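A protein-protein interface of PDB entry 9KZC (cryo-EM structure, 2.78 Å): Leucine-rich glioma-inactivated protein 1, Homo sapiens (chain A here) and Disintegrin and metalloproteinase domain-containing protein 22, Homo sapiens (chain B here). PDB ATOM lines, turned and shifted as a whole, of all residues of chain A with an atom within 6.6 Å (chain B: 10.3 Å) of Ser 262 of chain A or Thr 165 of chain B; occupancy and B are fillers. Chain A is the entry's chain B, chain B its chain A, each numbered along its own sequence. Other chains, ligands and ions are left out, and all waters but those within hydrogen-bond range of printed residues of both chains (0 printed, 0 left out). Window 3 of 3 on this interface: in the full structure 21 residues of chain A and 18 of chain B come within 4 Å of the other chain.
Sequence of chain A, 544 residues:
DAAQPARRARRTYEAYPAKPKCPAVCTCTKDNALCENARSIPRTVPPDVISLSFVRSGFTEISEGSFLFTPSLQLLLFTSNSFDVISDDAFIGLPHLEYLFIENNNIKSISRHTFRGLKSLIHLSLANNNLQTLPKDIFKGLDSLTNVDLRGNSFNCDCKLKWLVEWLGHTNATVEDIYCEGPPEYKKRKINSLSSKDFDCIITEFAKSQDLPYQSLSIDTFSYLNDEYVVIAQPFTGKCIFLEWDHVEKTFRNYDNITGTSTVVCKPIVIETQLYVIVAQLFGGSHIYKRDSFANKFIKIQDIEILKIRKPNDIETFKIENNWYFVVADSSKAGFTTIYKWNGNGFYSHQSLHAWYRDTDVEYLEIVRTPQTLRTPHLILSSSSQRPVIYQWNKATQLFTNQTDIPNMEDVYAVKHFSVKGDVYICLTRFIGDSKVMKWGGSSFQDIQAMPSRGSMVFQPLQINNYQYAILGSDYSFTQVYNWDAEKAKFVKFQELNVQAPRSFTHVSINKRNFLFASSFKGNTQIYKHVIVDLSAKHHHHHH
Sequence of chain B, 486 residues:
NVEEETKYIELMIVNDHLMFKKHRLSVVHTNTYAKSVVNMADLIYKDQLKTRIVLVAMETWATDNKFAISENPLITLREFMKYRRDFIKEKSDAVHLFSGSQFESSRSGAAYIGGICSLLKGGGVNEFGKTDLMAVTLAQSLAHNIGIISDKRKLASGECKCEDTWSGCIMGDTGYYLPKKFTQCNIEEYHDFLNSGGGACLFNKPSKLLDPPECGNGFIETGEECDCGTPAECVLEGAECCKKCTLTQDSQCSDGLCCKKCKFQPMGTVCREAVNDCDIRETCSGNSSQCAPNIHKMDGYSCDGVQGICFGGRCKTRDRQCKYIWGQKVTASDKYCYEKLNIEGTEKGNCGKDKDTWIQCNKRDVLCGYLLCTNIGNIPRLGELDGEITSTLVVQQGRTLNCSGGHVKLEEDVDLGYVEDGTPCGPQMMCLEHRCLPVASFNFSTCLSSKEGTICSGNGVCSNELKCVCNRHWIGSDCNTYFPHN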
ATOM      1  N   GLN A 234     -17.976 -13.082 -20.401  1.00  0.00           N
ATOM      2  CA  GLN A 234     -19.100 -13.204 -19.486  1.00  0.00           C
ATOM      3  C   GLN A 234     -18.666 -12.751 -18.099  1.00  0.00           C
ATOM      4  O   GLN A 234     -17.788 -13.386 -17.501  1.00  0.00           O
ATOM      5  CB  GLN A 234     -19.612 -14.633 -19.448  1.00  0.00           C
ATOM      6  CG  GLN A 234     -20.845 -14.821 -18.589  1.00  0.00           C
ATOM      7  CD  GLN A 234     -21.362 -16.241 -18.623  1.00  0.00           C
ATOM      8  OE1 GLN A 234     -20.777 -17.112 -19.264  1.00  0.00           O
ATOM      9  NE2 GLN A 234     -22.480 -16.480 -17.947  1.00  0.00           N
ATOM     10  N   PRO A 235     -19.237 -11.671 -17.559  1.00  0.00           N
ATOM     11  CA  PRO A 235     -18.630 -11.048 -16.370  1.00  0.00           C
ATOM     12  C   PRO A 235     -18.764 -11.872 -15.105  1.00  0.00           C
ATOM     13  O   PRO A 235     -17.782 -12.036 -14.373  1.00  0.00           O
ATOM     14  CB  PRO A 235     -19.397  -9.724 -16.249  1.00  0.00           C
ATOM     15  CG  PRO A 235     -19.960  -9.475 -17.598  1.00  0.00           C
ATOM     16  CD  PRO A 235     -20.279 -10.822 -18.154  1.00  0.00           C
ATOM     17  N   PHE A 236     -19.954 -12.396 -14.825  1.00  0.00           N
ATOM     18  CA  PHE A 236     -20.270 -12.916 -13.503  1.00  0.00           C
ATOM     19  C   PHE A 236     -19.911 -14.385 -13.326  1.00  0.00           C
ATOM     20  O   PHE A 236     -20.011 -14.898 -12.207  1.00  0.00           O
ATOM     21  CB  PHE A 236     -21.756 -12.698 -13.211  1.00  0.00           C
ATOM     22  CG  PHE A 236     -22.194 -11.272 -13.384  1.00  0.00           C
ATOM     23  CD1 PHE A 236     -21.550 -10.251 -12.702  1.00  0.00           C
ATOM     24  CD2 PHE A 236     -23.231 -10.947 -14.241  1.00  0.00           C
ATOM     25  CE1 PHE A 236     -21.940  -8.937 -12.862  1.00  0.00           C
ATOM     26  CE2 PHE A 236     -23.627  -9.634 -14.405  1.00  0.00           C
ATOM     27  CZ  PHE A 236     -22.981  -8.628 -13.714  1.00  0.00           C
ATOM     28  N   THR A 237     -19.497 -15.070 -14.390  1.00  0.00           N
ATOM     29  CA  THR A 237     -18.944 -16.409 -14.275  1.00  0.00           C
ATOM     30  C   THR A 237     -17.448 -16.455 -14.545  1.00  0.00           C
ATOM     31  O   THR A 237     -16.833 -17.509 -14.353  1.00  0.00           O
ATOM     32  CB  THR A 237     -19.662 -17.372 -15.227  1.00  0.00           C
ATOM     33  OG1 THR A 237     -19.289 -17.079 -16.578  1.00  0.00           O
ATOM     34  CG2 THR A 237     -21.167 -17.243 -15.076  1.00  0.00           C
ATOM     35  N   GLY A 238     -16.853 -15.344 -14.974  1.00  0.00           N
ATOM     36  CA  GLY A 238     -15.434 -15.295 -15.262  1.00  0.00           C
ATOM     37  C   GLY A 238     -15.032 -16.213 -16.393  1.00  0.00           C
ATOM     38  O   GLY A 238     -14.219 -17.122 -16.205  1.00  0.00           O
ATOM     39  N   LYS A 239     -15.597 -15.990 -17.576  1.00  0.00           N
ATOM     40  CA  LYS A 239     -15.347 -16.843 -18.728  1.00  0.00           C
ATOM     41  C   LYS A 239     -15.169 -15.993 -19.974  1.00  0.00           C
ATOM     42  O   LYS A 239     -15.915 -15.038 -20.197  1.00  0.00           O
ATOM     43  CB  LYS A 239     -16.497 -17.835 -18.950  1.00  0.00           C
ATOM     44  CG  LYS A 239     -16.591 -18.939 -17.915  1.00  0.00           C
ATOM     45  CD  LYS A 239     -16.010 -20.238 -18.438  1.00  0.00           C
ATOM     46  CE  LYS A 239     -16.311 -21.391 -17.495  1.00  0.00           C
ATOM     47  NZ  LYS A 239     -15.706 -22.669 -17.962  1.00  0.00           N
ATOM     48  N   GLY A 260     -11.711 -17.397 -15.940  1.00  0.00           N
ATOM     49  CA  GLY A 260     -11.161 -16.385 -15.062  1.00  0.00           C
ATOM     50  C   GLY A 260     -12.000 -16.243 -13.810  1.00  0.00           C
ATOM     51  O   GLY A 260     -12.692 -17.185 -13.419  1.00  0.00           O
ATOM     52  N   THR A 261     -11.949 -15.077 -13.167  1.00  0.00           N
ATOM     53  CA  THR A 261     -12.778 -14.808 -11.999  1.00  0.00           C
ATOM     54  C   THR A 261     -13.804 -13.717 -12.272  1.00  0.00           C
ATOM     55  O   THR A 261     -15.008 -13.950 -12.131  1.00  0.00           O
ATOM     56  CB  THR A 261     -11.900 -14.427 -10.799  1.00  0.00           C
ATOM     57  OG1 THR A 261     -11.300 -13.147 -11.032  1.00  0.00           O
ATOM     58  CG2 THR A 261     -10.806 -15.463 -10.588  1.00  0.00           C
ATOM     59  N   SER A 262     -13.358 -12.523 -12.665  1.00  0.00           N
ATOM     60  CA  SER A 262     -14.258 -11.440 -13.072  1.00  0.00           C
ATOM     61  C   SER A 262     -13.649 -10.793 -14.314  1.00  0.00           C
ATOM     62  O   SER A 262     -12.932  -9.796 -14.212  1.00  0.00           O
ATOM     63  CB  SER A 262     -14.455 -10.432 -11.948  1.00  0.00           C
ATOM     64  OG  SER A 262     -14.957 -11.058 -10.782  1.00  0.00           O
ATOM     65  N   THR A 263     -13.961 -11.347 -15.481  1.00  0.00           N
ATOM     66  CA  THR A 263     -13.363 -10.895 -16.730  1.00  0.00           C
ATOM     67  C   THR A 263     -14.219  -9.798 -17.349  1.00  0.00           C
ATOM     68  O   THR A 263     -15.431  -9.967 -17.518  1.00  0.00           O
ATOM     69  CB  THR A 263     -13.202 -12.055 -17.713  1.00  0.00           C
ATOM     70  OG1 THR A 263     -14.446 -12.294 -18.380  1.00  0.00           O
ATOM     71  CG2 THR A 263     -12.773 -13.315 -16.981  1.00  0.00           C
ATOM     72  N   VAL A 264     -13.582  -8.679 -17.686  1.00  0.00           N
ATOM     73  CA  VAL A 264     -14.281  -7.548 -18.284  1.00  0.00           C
ATOM     74  C   VAL A 264     -14.002  -7.502 -19.780  1.00  0.00           C
ATOM     75  O   VAL A 264     -14.880  -7.151 -20.574  1.00  0.00           O
ATOM     76  CB  VAL A 264     -13.889  -6.224 -17.600  1.00  0.00           C
ATOM     77  CG1 VAL A 264     -14.510  -6.139 -16.226  1.00  0.00           C
ATOM     78  CG2 VAL A 264     -12.379  -6.103 -17.490  1.00  0.00           C
ATOM     79  N   VAL A 265     -12.779  -7.851 -20.176  1.00  0.00           N
ATOM     80  CA  VAL A 265     -12.357  -7.795 -21.571  1.00  0.00           C
ATOM     81  C   VAL A 265     -11.588  -9.067 -21.902  1.00  0.00           C
ATOM     82  O   VAL A 265     -10.810  -9.564 -21.082  1.00  0.00           O
ATOM     83  CB  VAL A 265     -11.484  -6.552 -21.864  1.00  0.00           C
ATOM     84  CG1 VAL A 265     -11.352  -6.337 -23.361  1.00  0.00           C
ATOM     85  CG2 VAL A 265     -12.043  -5.306 -21.193  1.00  0.00           C
ATOM     86  N   ALA A 280      -8.574  -9.230 -19.296  1.00  0.00           N
ATOM     87  CA  ALA A 280      -8.554  -8.261 -18.210  1.00  0.00           C
ATOM     88  C   ALA A 280      -9.553  -8.686 -17.144  1.00  0.00           C
ATOM     89  O   ALA A 280     -10.718  -8.954 -17.452  1.00  0.00           O
ATOM     90  CB  ALA A 280      -8.886  -6.859 -18.719  1.00  0.00           C
ATOM     91  N   GLN A 281      -9.096  -8.744 -15.897  1.00  0.00           N
ATOM     92  CA  GLN A 281      -9.921  -9.206 -14.792  1.00  0.00           C
ATOM     93  C   GLN A 281      -9.954  -8.162 -13.689  1.00  0.00           C
ATOM     94  O   GLN A 281      -8.931  -7.554 -13.365  1.00  0.00           O
ATOM     95  CB  GLN A 281      -9.407 -10.534 -14.234  1.00  0.00           C
ATOM     96  CG  GLN A 281      -9.532 -11.698 -15.196  1.00  0.00           C
ATOM     97  CD  GLN A 281      -8.767 -12.918 -14.732  1.00  0.00           C
ATOM     98  OE1 GLN A 281      -8.608 -13.147 -13.535  1.00  0.00           O
ATOM     99  NE2 GLN A 281      -8.284 -13.707 -15.683  1.00  0.00           N
ATOM    100  N   LEU A 282     -11.141  -7.959 -13.114  1.00  0.00           N
ATOM    101  CA  LEU A 282     -11.267  -7.062 -11.973  1.00  0.00           C
ATOM    102  C   LEU A 282     -10.707  -7.692 -10.707  1.00  0.00           C
ATOM    103  O   LEU A 282     -10.276  -6.975  -9.797  1.00  0.00           O
ATOM    104  CB  LEU A 282     -12.730  -6.671 -11.769  1.00  0.00           C
ATOM    105  CG  LEU A 282     -13.311  -5.666 -12.764  1.00  0.00           C
ATOM    106  CD1 LEU A 282     -14.713  -5.258 -12.357  1.00  0.00           C
ATOM    107  CD2 LEU A 282     -12.410  -4.450 -12.891  1.00  0.00           C
ATOM    108  N   PHE A 283     -10.705  -9.020 -10.630  1.00  0.00           N
ATOM    109  CA  PHE A 283     -10.187  -9.748  -9.483  1.00  0.00           C
ATOM    110  C   PHE A 283      -9.198 -10.801  -9.958  1.00  0.00           C
ATOM    111  O   PHE A 283      -9.441 -11.489 -10.954  1.00  0.00           O
ATOM    112  CB  PHE A 283     -11.321 -10.410  -8.690  1.00  0.00           C
ATOM    113  CG  PHE A 283     -10.864 -11.111  -7.441  1.00  0.00           C
ATOM    114  CD1 PHE A 283     -10.662 -10.403  -6.269  1.00  0.00           C
ATOM    115  CD2 PHE A 283     -10.645 -12.479  -7.438  1.00  0.00           C
ATOM    116  CE1 PHE A 283     -10.243 -11.044  -5.119  1.00  0.00           C
ATOM    117  CE2 PHE A 283     -10.225 -13.125  -6.292  1.00  0.00           C
ATOM    118  CZ  PHE A 283     -10.025 -12.407  -5.131  1.00  0.00           C
ATOM    119  N   GLY A 284      -8.085 -10.924  -9.241  1.00  0.00           N
ATOM    120  CA  GLY A 284      -7.082 -11.920  -9.551  1.00  0.00           C
ATOM    121  C   GLY A 284      -6.068 -11.528 -10.601  1.00  0.00           C
ATOM    122  O   GLY A 284      -5.256 -12.373 -10.996  1.00  0.00           O
ATOM    123  N   LYS A 311      -7.818  -1.990 -12.002  1.00  0.00           N
ATOM    124  CA  LYS A 311      -9.240  -1.979 -12.343  1.00  0.00           C
ATOM    125  C   LYS A 311      -9.390  -1.669 -13.826  1.00  0.00           C
ATOM    126  O   LYS A 311      -9.803  -0.568 -14.206  1.00  0.00           O
ATOM    127  CB  LYS A 311     -10.000  -0.961 -11.491  1.00  0.00           C
ATOM    128  CG  LYS A 311     -10.003  -1.272 -10.006  1.00  0.00           C
ATOM    129  CD  LYS A 311     -10.712  -2.583  -9.725  1.00  0.00           C
ATOM    130  CE  LYS A 311     -10.969  -2.765  -8.243  1.00  0.00           C
ATOM    131  NZ  LYS A 311     -12.011  -3.797  -7.994  1.00  0.00           N
ATOM    132  N   LYS B 161     -11.932 -12.207   3.394  1.00  0.00           N
ATOM    133  CA  LYS B 161     -11.889 -11.711   2.028  1.00  0.00           C
ATOM    134  C   LYS B 161     -13.232 -11.084   1.691  1.00  0.00           C
ATOM    135  O   LYS B 161     -14.273 -11.501   2.204  1.00  0.00           O
ATOM    136  CB  LYS B 161     -11.555 -12.842   1.037  1.00  0.00           C
ATOM    137  CG  LYS B 161     -11.448 -12.411  -0.418  1.00  0.00           C
ATOM    138  CD  LYS B 161     -10.977 -13.556  -1.301  1.00  0.00           C
ATOM    139  CE  LYS B 161     -12.061 -14.610  -1.470  1.00  0.00           C
ATOM    140  NZ  LYS B 161     -13.210 -14.104  -2.269  1.00  0.00           N
ATOM    141  N   CYS B 162     -13.199 -10.064   0.835  1.00  0.00           N
ATOM    142  CA  CYS B 162     -14.429  -9.404   0.421  1.00  0.00           C
ATOM    143  C   CYS B 162     -15.321 -10.383  -0.335  1.00  0.00           C
ATOM    144  O   CYS B 162     -14.859 -11.105  -1.222  1.00  0.00           O
ATOM    145  CB  CYS B 162     -14.109  -8.188  -0.449  1.00  0.00           C
ATOM    146  SG  CYS B 162     -15.557  -7.299  -1.069  1.00  0.00           S
ATOM    147  N   GLU B 163     -16.604 -10.407   0.028  1.00  0.00           N
ATOM    148  CA  GLU B 163     -17.541 -11.348  -0.575  1.00  0.00           C
ATOM    149  C   GLU B 163     -17.905 -10.987  -2.007  1.00  0.00           C
ATOM    150  O   GLU B 163     -18.471 -11.828  -2.712  1.00  0.00           O
ATOM    151  CB  GLU B 163     -18.813 -11.434   0.271  1.00  0.00           C
ATOM    152  CG  GLU B 163     -18.601 -12.036   1.651  1.00  0.00           C
ATOM    153  CD  GLU B 163     -18.210 -13.500   1.598  1.00  0.00           C
ATOM    154  OE1 GLU B 163     -18.653 -14.203   0.665  1.00  0.00           O
ATOM    155  OE2 GLU B 163     -17.457 -13.947   2.489  1.00  0.00           O
ATOM    156  N   ASP B 164     -17.599  -9.773  -2.452  1.00  0.00           N
ATOM    157  CA  ASP B 164     -17.893  -9.326  -3.807  1.00  0.00           C
ATOM    158  C   ASP B 164     -16.602  -9.311  -4.611  1.00  0.00           C
ATOM    159  O   ASP B 164     -15.690  -8.532  -4.311  1.00  0.00           O
ATOM    160  CB  ASP B 164     -18.539  -7.941  -3.799  1.00  0.00           C
ATOM    161  CG  ASP B 164     -19.369  -7.677  -5.038  1.00  0.00           C
ATOM    162  OD1 ASP B 164     -19.003  -8.177  -6.120  1.00  0.00           O
ATOM    163  OD2 ASP B 164     -20.389  -6.966  -4.929  1.00  0.00           O
ATOM    164  N   THR B 165     -16.525 -10.171  -5.624  1.00  0.00           N
ATOM    165  CA  THR B 165     -15.373 -10.207  -6.513  1.00  0.00           C
ATOM    166  C   THR B 165     -15.525  -9.287  -7.715  1.00  0.00           C
ATOM    167  O   THR B 165     -14.568  -9.128  -8.480  1.00  0.00           O
ATOM    168  CB  THR B 165     -15.121 -11.638  -7.002  1.00  0.00           C
ATOM    169  OG1 THR B 165     -16.335 -12.187  -7.528  1.00  0.00           O
ATOM    170  CG2 THR B 165     -14.629 -12.511  -5.860  1.00  0.00           C
ATOM    171  N   TRP B 166     -16.697  -8.678  -7.900  1.00  0.00           N
ATOM    172  CA  TRP B 166     -16.928  -7.787  -9.030  1.00  0.00           C
ATOM    173  C   TRP B 166     -16.662  -6.329  -8.665  1.00  0.00           C
ATOM    174  O   TRP B 166     -15.771  -5.690  -9.235  1.00  0.00           O
ATOM    175  CB  TRP B 166     -18.363  -7.951  -9.539  1.00  0.00           C
ATOM    176  CG  TRP B 166     -18.647  -7.124 -10.743  1.00  0.00           C
ATOM    177  CD1 TRP B 166     -19.450  -6.025 -10.816  1.00  0.00           C
ATOM    178  CD2 TRP B 166     -18.117  -7.321 -12.056  1.00  0.00           C
ATOM    179  NE1 TRP B 166     -19.458  -5.528 -12.095  1.00  0.00           N
ATOM    180  CE2 TRP B 166     -18.646  -6.307 -12.876  1.00  0.00           C
ATOM    181  CE3 TRP B 166     -17.248  -8.260 -12.619  1.00  0.00           C
ATOM    182  CZ2 TRP B 166     -18.335  -6.205 -14.227  1.00  0.00           C
ATOM    183  CZ3 TRP B 166     -16.941  -8.157 -13.957  1.00  0.00           C
ATOM    184  CH2 TRP B 166     -17.483  -7.137 -14.746  1.00  0.00           C
ATOM    185  N   SER B 167     -17.425  -5.796  -7.715  1.00  0.00           N
ATOM    186  CA  SER B 167     -17.278  -4.410  -7.295  1.00  0.00           C
ATOM    187  C   SER B 167     -16.307  -4.240  -6.139  1.00  0.00           C
ATOM    188  O   SER B 167     -15.999  -3.102  -5.771  1.00  0.00           O
ATOM    189  CB  SER B 167     -18.641  -3.834  -6.901  1.00  0.00           C
ATOM    190  OG  SER B 167     -19.526  -3.819  -8.007  1.00  0.00           O
ATOM    191  N   GLY B 168     -15.814  -5.334  -5.565  1.00  0.00           N
ATOM    192  CA  GLY B 168     -14.938  -5.219  -4.424  1.00  0.00           C
ATOM    193  C   GLY B 168     -15.695  -4.721  -3.204  1.00  0.00           C
ATOM    194  O   GLY B 168     -16.928  -4.728  -3.145  1.00  0.00           O
ATOM    195  N   CYS B 169     -14.929  -4.281  -2.216  1.00  0.00           N
ATOM    196  CA  CYS B 169     -15.477  -3.724  -0.991  1.00  0.00           C
ATOM    197  C   CYS B 169     -15.020  -2.279  -0.839  1.00  0.00           C
ATOM    198  O   CYS B 169     -14.179  -1.784  -1.593  1.00  0.00           O
ATOM    199  CB  CYS B 169     -15.076  -4.568   0.224  1.00  0.00           C
ATOM    200  SG  CYS B 169     -16.093  -6.056   0.447  1.00  0.00           S
ATOM    201  N   ASP B 173      -9.296  -0.318  -3.247  1.00  0.00           N
ATOM    202  CA  ASP B 173      -9.183   0.672  -4.309  1.00  0.00           C
ATOM    203  C   ASP B 173     -10.404   0.613  -5.217  1.00  0.00           C
ATOM    204  O   ASP B 173     -10.876  -0.466  -5.586  1.00  0.00           O
ATOM    205  CB  ASP B 173      -7.909   0.443  -5.122  1.00  0.00           C
ATOM    206  CG  ASP B 173      -6.652   0.754  -4.333  1.00  0.00           C
ATOM    207  OD1 ASP B 173      -6.712   1.620  -3.435  1.00  0.00           O
ATOM    208  OD2 ASP B 173      -5.605   0.134  -4.612  1.00  0.00           O
ATOM    209  N   TYR B 177     -16.634   0.210 -11.289  1.00  0.00           N
ATOM    210  CA  TYR B 177     -17.711  -0.478 -10.587  1.00  0.00           C
ATOM    211  C   TYR B 177     -17.541  -0.242  -9.092  1.00  0.00           C
ATOM    212  O   TYR B 177     -16.653  -0.821  -8.458  1.00  0.00           O
ATOM    213  CB  TYR B 177     -17.710  -1.964 -10.930  1.00  0.00           C
ATOM    214  CG  TYR B 177     -17.984  -2.231 -12.392  1.00  0.00           C
ATOM    215  CD1 TYR B 177     -19.272  -2.139 -12.899  1.00  0.00           C
ATOM    216  CD2 TYR B 177     -16.957  -2.556 -13.266  1.00  0.00           C
ATOM    217  CE1 TYR B 177     -19.532  -2.374 -14.232  1.00  0.00           C
ATOM    218  CE2 TYR B 177     -17.208  -2.793 -14.604  1.00  0.00           C
ATOM    219  CZ  TYR B 177     -18.498  -2.699 -15.080  1.00  0.00           C
ATOM    220  OH  TYR B 177     -18.756  -2.934 -16.410  1.00  0.00           O
ATOM    221  N   LEU B 178     -18.389   0.607  -8.536  1.00  0.00           N
ATOM    222  CA  LEU B 178     -18.233   1.072  -7.168  1.00  0.00           C
ATOM    223  C   LEU B 178     -18.662  -0.003  -6.174  1.00  0.00           C
ATOM    224  O   LEU B 178     -19.630  -0.727  -6.420  1.00  0.00           O
ATOM    225  CB  LEU B 178     -19.051   2.333  -6.939  1.00  0.00           C
ATOM    226  CG  LEU B 178     -18.802   3.453  -7.940  1.00  0.00           C
ATOM    227  CD1 LEU B 178     -19.775   4.555  -7.669  1.00  0.00           C
ATOM    228  CD2 LEU B 178     -17.383   3.964  -7.849  1.00  0.00           C
ATOM    229  N   PRO B 179     -17.965  -0.120  -5.050  1.00  0.00           N
ATOM    230  CA  PRO B 179     -18.383  -1.068  -4.015  1.00  0.00           C
ATOM    231  C   PRO B 179     -19.647  -0.604  -3.313  1.00  0.00           C
ATOM    232  O   PRO B 179     -20.047   0.560  -3.382  1.00  0.00           O
ATOM    233  CB  PRO B 179     -17.193  -1.090  -3.053  1.00  0.00           C
ATOM    234  CG  PRO B 179     -16.507   0.210  -3.274  1.00  0.00           C
ATOM    235  CD  PRO B 179     -16.692   0.539  -4.719  1.00  0.00           C
ATOM    236  N   LYS B 180     -20.284  -1.550  -2.624  1.00  0.00           N
ATOM    237  CA  LYS B 180     -21.518  -1.279  -1.905  1.00  0.00           C
ATOM    238  C   LYS B 180     -21.546  -1.836  -0.490  1.00  0.00           C
ATOM    239  O   LYS B 180     -22.425  -1.444   0.284  1.00  0.00           O
ATOM    240  CB  LYS B 180     -22.720  -1.844  -2.680  1.00  0.00           C
ATOM    241  CG  LYS B 180     -24.033  -1.129  -2.413  1.00  0.00           C
ATOM    242  CD  LYS B 180     -25.168  -1.757  -3.203  1.00  0.00           C
ATOM    243  CE  LYS B 180     -25.523  -3.130  -2.658  1.00  0.00           C
ATOM    244  NZ  LYS B 180     -26.229  -3.045  -1.351  1.00  0.00           N
ATOM    245  N   LYS B 181     -20.622  -2.721  -0.122  1.00  0.00           N
ATOM    246  CA  LYS B 181     -20.680  -3.413   1.155  1.00  0.00           C
ATOM    247  C   LYS B 181     -19.324  -3.386   1.844  1.00  0.00           C
ATOM    248  O   LYS B 181     -18.278  -3.301   1.196  1.00  0.00           O
ATOM    249  CB  LYS B 181     -21.139  -4.867   0.977  1.00  0.00           C
ATOM    250  CG  LYS B 181     -22.598  -5.014   0.578  1.00  0.00           C
ATOM    251  CD  LYS B 181     -23.013  -6.473   0.528  1.00  0.00           C
ATOM    252  CE  LYS B 181     -24.505  -6.614   0.276  1.00  0.00           C
ATOM    253  NZ  LYS B 181     -24.862  -6.333  -1.142  1.00  0.00           N
ATOM    254  N   THR B 183     -16.606  -5.431   4.376  1.00  0.00           N
ATOM    255  CA  THR B 183     -16.255  -6.791   4.749  1.00  0.00           C
ATOM    256  C   THR B 183     -16.697  -7.065   6.184  1.00  0.00           C
ATOM    257  O   THR B 183     -17.004  -6.153   6.956  1.00  0.00           O
ATOM    258  CB  THR B 183     -14.750  -7.029   4.615  1.00  0.00           C
ATOM    259  OG1 THR B 183     -14.073  -6.466   5.744  1.00  0.00           O
ATOM    260  CG2 THR B 183     -14.214  -6.396   3.351  1.00  0.00           C
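The backbone carbonyl oxygen (O) of Thr 165 of chain B is in hydrogen-bond range of the side-chain hydroxyl (OG) of Ser 262 of chain A.
Of the 16 printed residues of chain B, 4 touch a printed residue of chain A. Of the 18 printed residues of chain A, 6 touch a printed residue of chain B. Along chain A the printed residues that touch a printed residue of chain B span positions 235 to 311. Among the printed residues, 8 pairs touch across the chains. Among the printed residues, no Asp or Glu carboxylate lies within 4 Å of a Lys or Arg side-chain nitrogen of the other chain.
The backbone NH (N) of Trp 166 of chain B lies within hydrogen-bond range of the side-chain carboxylate (OD1) of Asp 164 of chain B (3.0 Å). The side-chain hydroxyl (OG1) of Thr 261 of chain A lies within hydrogen-bond range of the backbone carbonyl oxygen (O) of Phe 283 of chain A. N of Leu 282 of chain A lies within hydrogen-bond range of O of Ser 262 of chain A, 2.8 Å away. The backbone carbonyl oxygen (O) of Ala 280 of chain A lies within hydrogen-bond range of the backbone NH (N) of Val 264 of chain A. O of Phe 283 of chain A sits close to OE1 of Gln 281 of chain A, 3.2 Å away. The side-chain sulfur (SG) of Cys 162 of chain B forms a disulfide with the side-chain sulfur (SG) of Cys 169 of chain B (2.0 Å).
Of chain B, only Thr 165 and Trp 166 come within 4 Å of Ser 262 of chain A. Thr 165 of chain B touches just these residues of chain A: Ser 262 and Phe 283. Gly 260 of chain A touches none of the printed residues of chain B. No residue of chain B comes within 4 Å of Thr 263 of chain A. No residue of chain B comes within 4 Å of Gln 281 of chain A. Printed residues of chain B within 4 Å of Phe 283 of chain A: Thr 165 (3.5 Å). Of the printed residues of chain A, Asp 173 of chain B touches Lys 311 (3.5 Å). Of the printed residues of chain A, Trp 166 of chain B touches Pro 235 (3.6 Å), Ser 262 (3.6 Å), Val 264 (3.5 Å) and Leu 282 (3.3 Å). Printed residues of chain B within 4 Å of Lys 311 of chain A: Asp 173. Printed residues of chain B within 4 Å of Val 264 of chain A: Trp 166 (3.5 Å). Of the printed residues of chain B, Pro 235 of chain A touches Trp 166. Lys 181 of chain B touches none of the printed residues of chain A.
Pro 235 of chain A touches Trp 166 of chain B. CE3 of Trp 166 of chain B touches CB of Ser 262 of chain A, 3.6 Å away. Val 264 of chain A touches Trp 166 of chain B. Leu 282 of chain A touches Trp 166 of chain B (CD1 to O, 3.3 Å). Leu 282 of chain A touches Tyr 177 of chain B (CD1 to CD2, 3.6 Å). CB of Phe 283 of chain A touches O of Thr 165 of chain B, at 3.5 Å. Lys 311 of chain A touches Asp 173 of chain B.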
